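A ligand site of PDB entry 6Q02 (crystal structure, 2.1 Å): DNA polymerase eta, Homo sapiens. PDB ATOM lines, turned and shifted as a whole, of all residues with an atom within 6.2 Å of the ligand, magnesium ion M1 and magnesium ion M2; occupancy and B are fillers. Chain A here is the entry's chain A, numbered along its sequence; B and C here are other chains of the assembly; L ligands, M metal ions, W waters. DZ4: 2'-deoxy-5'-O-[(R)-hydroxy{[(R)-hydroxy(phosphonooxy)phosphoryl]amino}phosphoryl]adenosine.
O2G of the ligand sits at hydrogen-bond distance from OH of Tyr 55. N6 of the ligand lies within hydrogen-bond range of N3 of CAR 4 of chain C, at 3.3 Å. O2B of the ligand lies within hydrogen-bond range of N of Phe 20 (3.2 Å). N of Phe 21 lies within hydrogen-bond range of O3' of the ligand (3.0 Å). The side-chain amino group of Lys 234 lies within salt-bridge range of an oxygen (O2G) of the ligand (3.6 Å). The guanidinium group (NH1) of Arg 58 lies within salt-bridge range of an oxygen (O3G) of the ligand, at 3.3 Å. N of Cys 19 sits at hydrogen-bond distance from O2G of the ligand (2.9 Å). The guanidinium group (NH1) of Arg 64 is in salt-bridge range of an oxygen (O2A) of the ligand (3.9 Å).
NH1 of Arg 58 sits close to OH of Tyr 55 (3.3 Å). N1 of DA 5 of chain C lies close to N3 of DT 8 of chain B. O3' of DT 8 of chain B sits close to the side-chain hydroxyl (OG) of Ser 116 (3.1 Å). The backbone NH of Asp 118 sits close to the side-chain hydroxyl of Ser 116 (3.3 Å). The side-chain carboxylate (OD1) of Asp 18 is in salt-bridge range of the side-chain amino group (NZ) of Lys 234 (2.8 Å). The backbone carbonyl oxygen of Val 53 is in hydrogen-bond range of the guanidinium group of Arg 58, 3.0 Å away. The backbone carbonyl oxygen of Asp 16 is in hydrogen-bond range of the side-chain amino group of Lys 234, 3.3 Å away. The backbone NH (N) of Glu 119 lies close to the side-chain hydroxyl (OG) of Ser 116 (3.4 Å).
CA of Asp 18 touches O2G of the ligand, 3.4 Å away. Ile 51 touches the ligand (O to C2', 3.3 Å). CB of Ala 52 touches O3' of the ligand (3.7 Å). Ile 117 touches the ligand (CG2 to O4', 3.7 Å). DT 3 of chain C touches the ligand. C2 of DA 5 of chain C touches N1 of the ligand, 3.5 Å away. Hydrophobic or aromatic side chains within 4 Å of the ligand: Phe 20, Phe 21, Ile 51, Ala 52, Tyr 55 and Ile 117. The nearest printed residue that does not touch the ligand is Glu 119 (4.4 Å).
Three residues have an atom within 4 Å of magnesium ion M1: Asp 16, Met 17 and Asp 118. The nearest printed residue that does not touch magnesium ion M1 is Lys 234 (4.4 Å).
Ser 116 touches magnesium ion M2. Of the 27 residues printed, 5 come within 4 Å of magnesium ion M2.
OD1 of Asp 16 is bound to magnesium ion M1 (2.0 Å). O1B of the ligand binds magnesium ion M1. An oxygen (O1G) of the ligand binds magnesium ion M1, 2.1 Å away. OD2 of Asp 118 binds magnesium ion M1. An oxygen (O1A) of the ligand is bound to magnesium ion M1. O of Met 17 binds magnesium ion M1 (2.3 Å).
Magnesium ion M2 is bound by the side-chain carboxylate (OD1) of Asp 118, at 2.1 Å. OE2 of Glu 119 is bound to magnesium ion M2, at 2.1 Å. Water W4 binds magnesium ion M2 (2.1 Å). OD2 of Asp 16 is bound to magnesium ion M2 (2.2 Å). O1A of the ligand is bound to magnesium ion M2 (2.4 Å). Magnesium ion M2 is bound by O3' of DT 8 of chain B (2.5 Å). Magnesium ion M2 has six donor atoms within binding distance.
Water W2 lies within hydrogen-bond range of N of Val 53, NH2 of Arg 58 and O2B of the ligand. Water W3 lies within hydrogen-bond range of the guanidinium group (NH1) of Arg 64, the backbone carbonyl oxygen (O) of Ile 51 and a nitrogen (N3A) of the ligand.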
ATOM      1  N   VAL A  15      18.668  -8.613   6.195  1.00  0.00           N
ATOM      2  CA  VAL A  15      17.253  -8.306   6.236  1.00  0.00           C
ATOM      3  C   VAL A  15      16.617  -9.145   7.342  1.00  0.00           C
ATOM      4  O   VAL A  15      16.897 -10.349   7.450  1.00  0.00           O
ATOM      5  CB  VAL A  15      16.575  -8.581   4.887  1.00  0.00           C
ATOM      6  CG1 VAL A  15      15.078  -8.299   4.955  1.00  0.00           C
ATOM      7  CG2 VAL A  15      17.231  -7.746   3.789  1.00  0.00           C
ATOM      8  N   ASP A  16      15.783  -8.527   8.166  1.00  0.00           N
ATOM      9  CA  ASP A  16      15.107  -9.210   9.258  1.00  0.00           C
ATOM     10  C   ASP A  16      13.662  -8.765   9.311  1.00  0.00           C
ATOM     11  O   ASP A  16      13.384  -7.561   9.437  1.00  0.00           O
ATOM     12  CB  ASP A  16      15.807  -8.936  10.602  1.00  0.00           C
ATOM     13  CG  ASP A  16      15.149  -9.657  11.761  1.00  0.00           C
ATOM     14  OD1 ASP A  16      13.919  -9.544  11.920  1.00  0.00           O
ATOM     15  OD2 ASP A  16      15.869 -10.357  12.511  1.00  0.00           O
ATOM     16  N   MET A  17      12.743  -9.714   9.227  1.00  0.00           N
ATOM     17  CA  MET A  17      11.315  -9.395   9.268  1.00  0.00           C
ATOM     18  C   MET A  17      10.943  -8.854  10.635  1.00  0.00           C
ATOM     19  O   MET A  17      11.380  -9.365  11.669  1.00  0.00           O
ATOM     20  CB  MET A  17      10.487 -10.647   8.952  1.00  0.00           C
ATOM     21  CG  MET A  17      10.933 -11.393   7.702  1.00  0.00           C
ATOM     22  SD  MET A  17      11.064 -10.333   6.255  1.00  0.00           S
ATOM     23  CE  MET A  17       9.400  -9.716   6.108  1.00  0.00           C
ATOM     24  N   ASP A  18      10.118  -7.807  10.637  1.00  0.00           N
ATOM     25  CA  ASP A  18       9.624  -7.227  11.880  1.00  0.00           C
ATOM     26  C   ASP A  18       8.549  -8.123  12.475  1.00  0.00           C
ATOM     27  O   ASP A  18       7.655  -8.582  11.766  1.00  0.00           O
ATOM     28  CB  ASP A  18       9.060  -5.824  11.621  1.00  0.00           C
ATOM     29  CG  ASP A  18      10.081  -4.891  11.000  1.00  0.00           C
ATOM     30  OD1 ASP A  18      11.293  -5.070  11.269  1.00  0.00           O
ATOM     31  OD2 ASP A  18       9.678  -3.977  10.257  1.00  0.00           O
ATOM     32  N   CYS A  19       8.646  -8.370  13.789  1.00  0.00           N
ATOM     33  CA  CYS A  19       7.772  -9.295  14.511  1.00  0.00           C
ATOM     34  C   CYS A  19       7.147 -10.318  13.570  1.00  0.00           C
ATOM     35  O   CYS A  19       5.941 -10.271  13.301  1.00  0.00           O
ATOM     36  CB  CYS A  19       6.689  -8.524  15.272  1.00  0.00           C
ATOM     37  SG  CYS A  19       5.774  -7.305  14.316  1.00  0.00           S
ATOM     38  N   PHE A  20       7.960 -11.258  13.080  1.00  0.00           N
ATOM     39  CA  PHE A  20       7.594 -12.032  11.899  1.00  0.00           C
ATOM     40  C   PHE A  20       6.326 -12.851  12.129  1.00  0.00           C
ATOM     41  O   PHE A  20       5.346 -12.719  11.396  1.00  0.00           O
ATOM     42  CB  PHE A  20       8.750 -12.941  11.480  1.00  0.00           C
ATOM     43  CG  PHE A  20       8.486 -13.690  10.215  1.00  0.00           C
ATOM     44  CD1 PHE A  20       7.974 -13.047   9.099  1.00  0.00           C
ATOM     45  CD2 PHE A  20       8.749 -15.052  10.125  1.00  0.00           C
ATOM     46  CE1 PHE A  20       7.731 -13.737   7.937  1.00  0.00           C
ATOM     47  CE2 PHE A  20       8.506 -15.742   8.963  1.00  0.00           C
ATOM     48  CZ  PHE A  20       7.989 -15.089   7.863  1.00  0.00           C
ATOM     49  N   PHE A  21       6.333 -13.719  13.140  1.00  0.00           N
ATOM     50  CA  PHE A  21       5.167 -14.580  13.366  1.00  0.00           C
ATOM     51  C   PHE A  21       3.911 -13.753  13.550  1.00  0.00           C
ATOM     52  O   PHE A  21       2.825 -14.147  13.109  1.00  0.00           O
ATOM     53  CB  PHE A  21       5.399 -15.491  14.570  1.00  0.00           C
ATOM     54  CG  PHE A  21       6.365 -16.627  14.325  1.00  0.00           C
ATOM     55  CD1 PHE A  21       7.308 -16.554  13.312  1.00  0.00           C
ATOM     56  CD2 PHE A  21       6.337 -17.750  15.122  1.00  0.00           C
ATOM     57  CE1 PHE A  21       8.199 -17.594  13.094  1.00  0.00           C
ATOM     58  CE2 PHE A  21       7.226 -18.794  14.917  1.00  0.00           C
ATOM     59  CZ  PHE A  21       8.158 -18.714  13.897  1.00  0.00           C
ATOM     60  N   VAL A  22       4.030 -12.594  14.203  1.00  0.00           N
ATOM     61  CA  VAL A  22       2.871 -11.727  14.378  1.00  0.00           C
ATOM     62  C   VAL A  22       2.367 -11.237  13.032  1.00  0.00           C
ATOM     63  O   VAL A  22       1.147 -11.233  12.774  1.00  0.00           O
ATOM     64  CB  VAL A  22       3.238 -10.550  15.314  1.00  0.00           C
ATOM     65  CG1 VAL A  22       2.193  -9.449  15.264  1.00  0.00           C
ATOM     66  CG2 VAL A  22       3.382 -11.067  16.742  1.00  0.00           C
ATOM     67  N   GLN A  41       2.315 -20.076  22.215  1.00  0.00           N
ATOM     68  CA  GLN A  41       2.516 -21.509  22.028  1.00  0.00           C
ATOM     69  C   GLN A  41       1.793 -22.238  23.148  1.00  0.00           C
ATOM     70  O   GLN A  41       2.111 -22.037  24.327  1.00  0.00           O
ATOM     71  CB  GLN A  41       4.011 -21.834  22.023  1.00  0.00           C
ATOM     72  CG  GLN A  41       4.415 -22.998  21.163  1.00  0.00           C
ATOM     73  CD  GLN A  41       5.875 -22.928  20.760  1.00  0.00           C
ATOM     74  OE1 GLN A  41       6.227 -23.199  19.618  1.00  0.00           O
ATOM     75  NE2 GLN A  41       6.734 -22.536  21.697  1.00  0.00           N
ATOM     76  N   ILE A  51       6.045 -16.168  21.920  1.00  0.00           N
ATOM     77  CA  ILE A  51       7.234 -16.275  21.072  1.00  0.00           C
ATOM     78  C   ILE A  51       7.378 -15.113  20.101  1.00  0.00           C
ATOM     79  O   ILE A  51       8.432 -14.992  19.470  1.00  0.00           O
ATOM     80  CB  ILE A  51       7.264 -17.614  20.309  1.00  0.00           C
ATOM     81  CG1 ILE A  51       5.994 -17.780  19.459  1.00  0.00           C
ATOM     82  CG2 ILE A  51       7.421 -18.780  21.286  1.00  0.00           C
ATOM     83  CD1 ILE A  51       6.003 -19.027  18.583  1.00  0.00           C
ATOM     84  N   ALA A  52       6.367 -14.253  19.958  1.00  0.00           N
ATOM     85  CA  ALA A  52       6.456 -13.098  19.074  1.00  0.00           C
ATOM     86  C   ALA A  52       5.482 -12.036  19.571  1.00  0.00           C
ATOM     87  O   ALA A  52       4.393 -12.355  20.037  1.00  0.00           O
ATOM     88  CB  ALA A  52       6.138 -13.483  17.621  1.00  0.00           C
ATOM     89  N   VAL A  53       5.896 -10.775  19.452  1.00  0.00           N
ATOM     90  CA  VAL A  53       5.182  -9.659  20.066  1.00  0.00           C
ATOM     91  C   VAL A  53       5.132  -8.502  19.078  1.00  0.00           C
ATOM     92  O   VAL A  53       6.179  -8.078  18.557  1.00  0.00           O
ATOM     93  CB  VAL A  53       5.842  -9.217  21.377  1.00  0.00           C
ATOM     94  CG1 VAL A  53       5.001  -8.154  22.073  1.00  0.00           C
ATOM     95  CG2 VAL A  53       6.064 -10.401  22.300  1.00  0.00           C
ATOM     96  N   TYR A  55       4.844  -4.608  17.906  1.00  0.00           N
ATOM     97  CA  TYR A  55       5.465  -3.418  18.482  1.00  0.00           C
ATOM     98  C   TYR A  55       4.467  -2.601  19.301  1.00  0.00           C
ATOM     99  O   TYR A  55       4.862  -1.922  20.246  1.00  0.00           O
ATOM    100  CB  TYR A  55       6.099  -2.574  17.384  1.00  0.00           C
ATOM    101  CG  TYR A  55       7.433  -3.118  16.945  1.00  0.00           C
ATOM    102  CD1 TYR A  55       7.529  -4.133  16.007  1.00  0.00           C
ATOM    103  CD2 TYR A  55       8.616  -2.624  17.486  1.00  0.00           C
ATOM    104  CE1 TYR A  55       8.755  -4.637  15.608  1.00  0.00           C
ATOM    105  CE2 TYR A  55       9.848  -3.124  17.109  1.00  0.00           C
ATOM    106  CZ  TYR A  55       9.903  -4.134  16.168  1.00  0.00           C
ATOM    107  OH  TYR A  55      11.136  -4.631  15.778  1.00  0.00           O
ATOM    108  N   ARG A  58       4.760  -4.370  22.590  1.00  0.00           N
ATOM    109  CA  ARG A  58       6.044  -4.154  23.242  1.00  0.00           C
ATOM    110  C   ARG A  58       6.057  -2.858  24.044  1.00  0.00           C
ATOM    111  O   ARG A  58       6.776  -2.749  25.047  1.00  0.00           O
ATOM    112  CB  ARG A  58       7.167  -4.138  22.209  1.00  0.00           C
ATOM    113  CG  ARG A  58       7.335  -5.435  21.436  1.00  0.00           C
ATOM    114  CD  ARG A  58       8.519  -5.374  20.478  1.00  0.00           C
ATOM    115  NE  ARG A  58       8.471  -6.470  19.512  1.00  0.00           N
ATOM    116  CZ  ARG A  58       9.461  -6.785  18.688  1.00  0.00           C
ATOM    117  NH1 ARG A  58      10.591  -6.088  18.691  1.00  0.00           N
ATOM    118  NH2 ARG A  58       9.323  -7.793  17.847  1.00  0.00           N
ATOM    119  N   ARG A  64       9.072 -11.587  24.426  1.00  0.00           N
ATOM    120  CA  ARG A  64       9.212 -13.010  24.154  1.00  0.00           C
ATOM    121  C   ARG A  64       9.522 -13.764  25.439  1.00  0.00           C
ATOM    122  O   ARG A  64      10.198 -13.260  26.336  1.00  0.00           O
ATOM    123  CB  ARG A  64      10.311 -13.228  23.117  1.00  0.00           C
ATOM    124  CG  ARG A  64      10.720 -14.675  22.880  1.00  0.00           C
ATOM    125  CD  ARG A  64      11.921 -14.761  21.936  1.00  0.00           C
ATOM    126  NE  ARG A  64      13.038 -13.928  22.398  1.00  0.00           N
ATOM    127  CZ  ARG A  64      13.580 -12.926  21.711  1.00  0.00           C
ATOM    128  NH1 ARG A  64      13.148 -12.601  20.504  1.00  0.00           N
ATOM    129  NH2 ARG A  64      14.591 -12.244  22.250  1.00  0.00           N
ATOM    130  N   LEU A  92       5.057 -25.444  13.149  1.00  0.00           N
ATOM    131  CA  LEU A  92       5.473 -24.141  12.659  1.00  0.00           C
ATOM    132  C   LEU A  92       5.432 -24.045  11.129  1.00  0.00           C
ATOM    133  O   LEU A  92       6.085 -23.173  10.558  1.00  0.00           O
ATOM    134  CB  LEU A  92       6.885 -23.821  13.160  1.00  0.00           C
ATOM    135  CG  LEU A  92       7.088 -23.986  14.673  1.00  0.00           C
ATOM    136  CD1 LEU A  92       8.561 -23.837  15.019  1.00  0.00           C
ATOM    137  CD2 LEU A  92       6.257 -22.977  15.432  1.00  0.00           C
ATOM    138  N   SER A 116      18.166 -17.471   9.487  1.00  0.00           N
ATOM    139  CA  SER A 116      17.150 -17.965  10.405  1.00  0.00           C
ATOM    140  C   SER A 116      15.829 -18.021   9.653  1.00  0.00           C
ATOM    141  O   SER A 116      15.783 -17.802   8.434  1.00  0.00           O
ATOM    142  CB  SER A 116      17.056 -17.076  11.658  1.00  0.00           C
ATOM    143  OG  SER A 116      16.400 -15.851  11.362  1.00  0.00           O
ATOM    144  N   ILE A 117      14.743 -18.307  10.368  1.00  0.00           N
ATOM    145  CA  ILE A 117      13.445 -18.398   9.707  1.00  0.00           C
ATOM    146  C   ILE A 117      12.981 -17.050   9.170  1.00  0.00           C
ATOM    147  O   ILE A 117      12.119 -17.017   8.290  1.00  0.00           O
ATOM    148  CB  ILE A 117      12.393 -18.994  10.655  1.00  0.00           C
ATOM    149  CG1 ILE A 117      11.108 -19.304   9.880  1.00  0.00           C
ATOM    150  CG2 ILE A 117      12.106 -18.047  11.824  1.00  0.00           C
ATOM    151  CD1 ILE A 117      10.100 -20.123  10.653  1.00  0.00           C
ATOM    152  N   ASP A 118      13.526 -15.930   9.670  1.00  0.00           N
ATOM    153  CA  ASP A 118      13.049 -14.616   9.248  1.00  0.00           C
ATOM    154  C   ASP A 118      14.169 -13.641   8.911  1.00  0.00           C
ATOM    155  O   ASP A 118      13.936 -12.434   8.889  1.00  0.00           O
ATOM    156  CB  ASP A 118      12.151 -13.994  10.320  1.00  0.00           C
ATOM    157  CG  ASP A 118      12.931 -13.196  11.354  1.00  0.00           C
ATOM    158  OD1 ASP A 118      14.031 -13.640  11.747  1.00  0.00           O
ATOM    159  OD2 ASP A 118      12.445 -12.129  11.774  1.00  0.00           O
ATOM    160  N   GLU A 119      15.380 -14.118   8.625  1.00  0.00           N
ATOM    161  CA  GLU A 119      16.417 -13.186   8.216  1.00  0.00           C
ATOM    162  C   GLU A 119      17.416 -13.882   7.308  1.00  0.00           C
ATOM    163  O   GLU A 119      17.613 -15.098   7.374  1.00  0.00           O
ATOM    164  CB  GLU A 119      17.130 -12.556   9.423  1.00  0.00           C
ATOM    165  CG  GLU A 119      17.975 -13.502  10.220  1.00  0.00           C
ATOM    166  CD  GLU A 119      18.060 -13.100  11.678  1.00  0.00           C
ATOM    167  OE1 GLU A 119      19.023 -12.406  12.061  1.00  0.00           O
ATOM    168  OE2 GLU A 119      17.137 -13.468  12.445  1.00  0.00           O
ATOM    169  N   LYS A 227      24.282  -6.903  10.457  1.00  0.00           N
ATOM    170  CA  LYS A 227      23.392  -7.330  11.529  1.00  0.00           C
ATOM    171  C   LYS A 227      23.218  -6.228  12.572  1.00  0.00           C
ATOM    172  O   LYS A 227      22.090  -5.843  12.906  1.00  0.00           O
ATOM    173  CB  LYS A 227      23.949  -8.610  12.173  1.00  0.00           C
ATOM    174  CG  LYS A 227      23.294  -9.030  13.494  1.00  0.00           C
ATOM    175  CD  LYS A 227      22.067  -9.887  13.283  1.00  0.00           C
ATOM    176  CE  LYS A 227      21.613 -10.515  14.590  1.00  0.00           C
ATOM    177  NZ  LYS A 227      20.210 -10.982  14.518  1.00  0.00           N
ATOM    178  N   LYS A 234      14.805  -0.284  14.144  1.00  0.00           N
ATOM    179  CA  LYS A 234      13.653  -1.142  13.919  1.00  0.00           C
ATOM    180  C   LYS A 234      12.398  -0.495  14.501  1.00  0.00           C
ATOM    181  O   LYS A 234      12.475   0.222  15.510  1.00  0.00           O
ATOM    182  CB  LYS A 234      13.877  -2.507  14.554  1.00  0.00           C
ATOM    183  CG  LYS A 234      14.030  -3.636  13.547  1.00  0.00           C
ATOM    184  CD  LYS A 234      14.705  -4.858  14.152  1.00  0.00           C
ATOM    185  CE  LYS A 234      13.895  -6.122  13.923  1.00  0.00           C
ATOM    186  NZ  LYS A 234      13.517  -6.335  12.500  1.00  0.00           N
ATOM    187  N   PRO A 235      11.224  -0.730  13.895  1.00  0.00           N
ATOM    188  CA  PRO A 235      10.915  -1.527  12.708  1.00  0.00           C
ATOM    189  C   PRO A 235      10.719  -0.725  11.426  1.00  0.00           C
ATOM    190  O   PRO A 235      10.628   0.505  11.456  1.00  0.00           O
ATOM    191  CB  PRO A 235       9.603  -2.201  13.089  1.00  0.00           C
ATOM    192  CG  PRO A 235       8.900  -1.149  13.895  1.00  0.00           C
ATOM    193  CD  PRO A 235       9.982  -0.340  14.596  1.00  0.00           C
ATOM    194  P    DT B   8      19.737 -13.310  17.507  1.00  0.00           P
ATOM    195  OP1  DT B   8      19.729 -12.041  16.754  1.00  0.00           O
ATOM    196  OP2  DT B   8      19.420 -13.312  18.957  1.00  0.00           O
ATOM    197  O5'  DT B   8      18.729 -14.341  16.824  1.00  0.00           O
ATOM    198  C5'  DT B   8      18.785 -14.573  15.422  1.00  0.00           C
ATOM    199  C4'  DT B   8      17.561 -15.335  14.955  1.00  0.00           C
ATOM    200  O4'  DT B   8      17.480 -16.596  15.678  1.00  0.00           O
ATOM    201  C3'  DT B   8      16.236 -14.614  15.187  1.00  0.00           C
ATOM    202  O3'  DT B   8      15.436 -14.633  14.004  1.00  0.00           O
ATOM    203  C2'  DT B   8      15.594 -15.361  16.342  1.00  0.00           C
ATOM    204  C1'  DT B   8      16.197 -16.759  16.242  1.00  0.00           C
ATOM    205  N1   DT B   8      16.325 -17.459  17.561  1.00  0.00           N
ATOM    206  C2   DT B   8      15.586 -18.597  17.799  1.00  0.00           C
ATOM    207  O2   DT B   8      14.821 -19.085  16.976  1.00  0.00           O
ATOM    208  N3   DT B   8      15.772 -19.156  19.033  1.00  0.00           N
ATOM    209  C4   DT B   8      16.607 -18.701  20.033  1.00  0.00           C
ATOM    210  O4   DT B   8      16.697 -19.274  21.112  1.00  0.00           O
ATOM    211  C5   DT B   8      17.343 -17.498  19.728  1.00  0.00           C
ATOM    212  C7   DT B   8      18.272 -16.913  20.747  1.00  0.00           C
ATOM    213  C6   DT B   8      17.173 -16.942  18.525  1.00  0.00           C
ATOM    214  P    DT C   3      10.107 -21.950  33.489  1.00  0.00           P
ATOM    215  OP1  DT C   3      10.615 -22.187  34.870  1.00  0.00           O
ATOM    216  OP2  DT C   3       9.817 -20.572  33.046  1.00  0.00           O
ATOM    217  O5'  DT C   3      11.141 -22.614  32.460  1.00  0.00           O
ATOM    218  C5'  DT C   3      11.265 -22.084  31.142  1.00  0.00           C
ATOM    219  C4'  DT C   3      10.056 -22.450  30.291  1.00  0.00           C
ATOM    220  O4'  DT C   3       9.759 -21.360  29.382  1.00  0.00           O
ATOM    221  C3'  DT C   3      10.238 -23.688  29.424  1.00  0.00           C
ATOM    222  O3'  DT C   3       9.035 -24.437  29.371  1.00  0.00           O
ATOM    223  C2'  DT C   3      10.631 -23.123  28.066  1.00  0.00           C
ATOM    224  C1'  DT C   3       9.917 -21.777  28.031  1.00  0.00           C
ATOM    225  N1   DT C   3      10.662 -20.709  27.289  1.00  0.00           N
ATOM    226  C2   DT C   3      11.908 -20.336  27.730  1.00  0.00           C
ATOM    227  O2   DT C   3      12.458 -20.837  28.692  1.00  0.00           O
ATOM    228  N3   DT C   3      12.504 -19.346  26.981  1.00  0.00           N
ATOM    229  C4   DT C   3      11.983 -18.714  25.868  1.00  0.00           C
ATOM    230  O4   DT C   3      12.600 -17.843  25.263  1.00  0.00           O
ATOM    231  C5   DT C   3      10.662 -19.155  25.461  1.00  0.00           C
ATOM    232  C7   DT C   3      10.003 -18.540  24.270  1.00  0.00           C
ATOM    233  C6   DT C   3      10.076 -20.124  26.187  1.00  0.00           C
ATOM    234  P   CAR C   4       9.003 -25.895  28.691  1.00  0.00           P
ATOM    235  OP1 CAR C   4       7.665 -26.492  29.064  1.00  0.00           O
ATOM    236  OP2 CAR C   4      10.285 -26.625  29.028  1.00  0.00           O
ATOM    237  O5' CAR C   4       8.968 -25.600  27.132  1.00  0.00           O
ATOM    238  C5' CAR C   4       7.850 -24.926  26.562  1.00  0.00           C
ATOM    239  C4' CAR C   4       8.018 -24.680  25.083  1.00  0.00           C
ATOM    240  O4' CAR C   4       8.880 -23.530  24.899  1.00  0.00           O
ATOM    241  C3' CAR C   4       8.656 -25.841  24.303  1.00  0.00           C
ATOM    242  O3' CAR C   4       7.803 -26.269  23.256  1.00  0.00           O
ATOM    243  C2' CAR C   4       9.941 -25.248  23.696  1.00  0.00           C
ATOM    244  O2' CAR C   4      11.140 -25.653  24.315  1.00  0.00           O
ATOM    245  C1' CAR C   4       9.692 -23.739  23.770  1.00  0.00           C
ATOM    246  N1  CAR C   4      10.909 -22.921  23.905  1.00  0.00           N
ATOM    247  C2  CAR C   4      11.197 -21.920  22.946  1.00  0.00           C
ATOM    248  O2  CAR C   4      10.422 -21.739  21.986  1.00  0.00           O
ATOM    249  N3  CAR C   4      12.305 -21.161  23.062  1.00  0.00           N
ATOM    250  C4  CAR C   4      13.160 -21.336  24.091  1.00  0.00           C
ATOM    251  N4  CAR C   4      14.278 -20.576  24.209  1.00  0.00           N
ATOM    252  C5  CAR C   4      12.900 -22.315  25.045  1.00  0.00           C
ATOM    253  C6  CAR C   4      11.751 -23.085  24.936  1.00  0.00           C
ATOM    254  P    DA C   5       8.089 -27.672  22.525  1.00  0.00           P
ATOM    255  OP1  DA C   5       6.801 -28.376  22.370  1.00  0.00           O
ATOM    256  OP2  DA C   5       9.211 -28.327  23.232  1.00  0.00           O
ATOM    257  O5'  DA C   5       8.623 -27.221  21.086  1.00  0.00           O
ATOM    258  C5'  DA C   5       7.827 -26.359  20.283  1.00  0.00           C
ATOM    259  C4'  DA C   5       8.620 -25.864  19.090  1.00  0.00           C
ATOM    260  O4'  DA C   5       9.557 -24.830  19.517  1.00  0.00           O
ATOM    261  C3'  DA C   5       9.454 -26.934  18.385  1.00  0.00           C
ATOM    262  O3'  DA C   5       9.294 -26.862  16.980  1.00  0.00           O
ATOM    263  C2'  DA C   5      10.885 -26.598  18.818  1.00  0.00           C
ATOM    264  C1'  DA C   5      10.806 -25.093  18.933  1.00  0.00           C
ATOM    265  N9   DA C   5      11.860 -24.499  19.751  1.00  0.00           N
ATOM    266  C8   DA C   5      12.329 -24.946  20.949  1.00  0.00           C
ATOM    267  N7   DA C   5      13.293 -24.200  21.446  1.00  0.00           N
ATOM    268  C5   DA C   5      13.465 -23.207  20.507  1.00  0.00           C
ATOM    269  C6   DA C   5      14.337 -22.099  20.438  1.00  0.00           C
ATOM    270  N6   DA C   5      15.233 -21.805  21.388  1.00  0.00           N
ATOM    271  N1   DA C   5      14.253 -21.301  19.351  1.00  0.00           N
ATOM    272  C2   DA C   5      13.354 -21.591  18.410  1.00  0.00           C
ATOM    273  N3   DA C   5      12.481 -22.595  18.363  1.00  0.00           N
ATOM    274  C4   DA C   5      12.593 -23.379  19.449  1.00  0.00           C
HETATM  275  N1  DZ4 L   1      11.282 -19.612  20.502  1.00  0.00           N
HETATM  276  C2  DZ4 L   1      10.368 -19.803  19.530  1.00  0.00           C
HETATM  277  N3  DZ4 L   1      10.263 -19.003  18.448  1.00  0.00           N
HETATM  278  C4  DZ4 L   1      11.100 -17.952  18.282  1.00  0.00           C
HETATM  279  C5  DZ4 L   1      12.125 -17.684  19.300  1.00  0.00           C
HETATM  280  C6  DZ4 L   1      12.168 -18.603  20.465  1.00  0.00           C
HETATM  281  N6  DZ4 L   1      13.092 -18.410  21.439  1.00  0.00           N
HETATM  282  N7  DZ4 L   1      12.808 -16.603  18.911  1.00  0.00           N
HETATM  283  C8  DZ4 L   1      12.283 -16.204  17.739  1.00  0.00           C
HETATM  284  N9  DZ4 L   1      11.268 -16.999  17.356  1.00  0.00           N
HETATM  285  PA  DZ4 L   1      13.265 -12.510  15.839  1.00  0.00           P
HETATM  286  PB  DZ4 L   1      10.755 -10.848  15.640  1.00  0.00           P
HETATM  287  PG  DZ4 L   1      11.822  -8.269  15.508  1.00  0.00           P
HETATM  288  C1' DZ4 L   1      10.460 -16.842  16.131  1.00  0.00           C
HETATM  289  O1A DZ4 L   1      13.720 -11.810  14.622  1.00  0.00           O
HETATM  290  O1B DZ4 L   1      11.038 -10.997  14.203  1.00  0.00           O
HETATM  291  O1G DZ4 L   1      12.609  -9.054  14.495  1.00  0.00           O
HETATM  292  C2' DZ4 L   1       9.386 -15.802  16.392  1.00  0.00           C
HETATM  293  O2A DZ4 L   1      14.468 -12.679  16.884  1.00  0.00           O
HETATM  294  O2B DZ4 L   1       9.350 -11.552  15.988  1.00  0.00           O
HETATM  295  O2G DZ4 L   1      11.012  -7.130  14.941  1.00  0.00           O
HETATM  296  C3' DZ4 L   1       9.799 -14.578  15.586  1.00  0.00           C
HETATM  297  O3' DZ4 L   1       8.671 -13.940  14.998  1.00  0.00           O
HETATM  298  N3A DZ4 L   1      11.990 -11.617  16.612  1.00  0.00           N
HETATM  299  O3B DZ4 L   1      10.709  -9.297  16.054  1.00  0.00           O
HETATM  300  O3G DZ4 L   1      12.605  -7.919  16.756  1.00  0.00           O
HETATM  301  C4' DZ4 L   1      10.769 -15.122  14.547  1.00  0.00           C
HETATM  302  O4' DZ4 L   1      11.276 -16.359  15.062  1.00  0.00           O
HETATM  303  C5' DZ4 L   1      11.914 -14.167  14.266  1.00  0.00           C
HETATM  304  O5' DZ4 L   1      12.687 -13.961  15.444  1.00  0.00           O
HETATM  305 MG    MG M   1      12.707 -10.584  13.129  1.00  0.00          MG
HETATM  306 MG    MG M   2      15.337 -12.440  12.913  1.00  0.00          MG
HETATM  307  O   HOH W   1       9.233 -20.899  16.671  1.00  0.00           O
HETATM  308  O   HOH W   2       8.550 -10.360  18.732  1.00  0.00           O
HETATM  309  O   HOH W   3      10.829 -13.240  19.018  1.00  0.00           O
HETATM  310  O   HOH W   4      15.985 -11.254  14.565  1.00  0.00           O
HETATM  311  O   HOH W   5      15.369  -9.017  15.814  1.00  0.00           O
HETATM  312  O   HOH W   6      12.865  -9.310  18.863  1.00  0.00           O
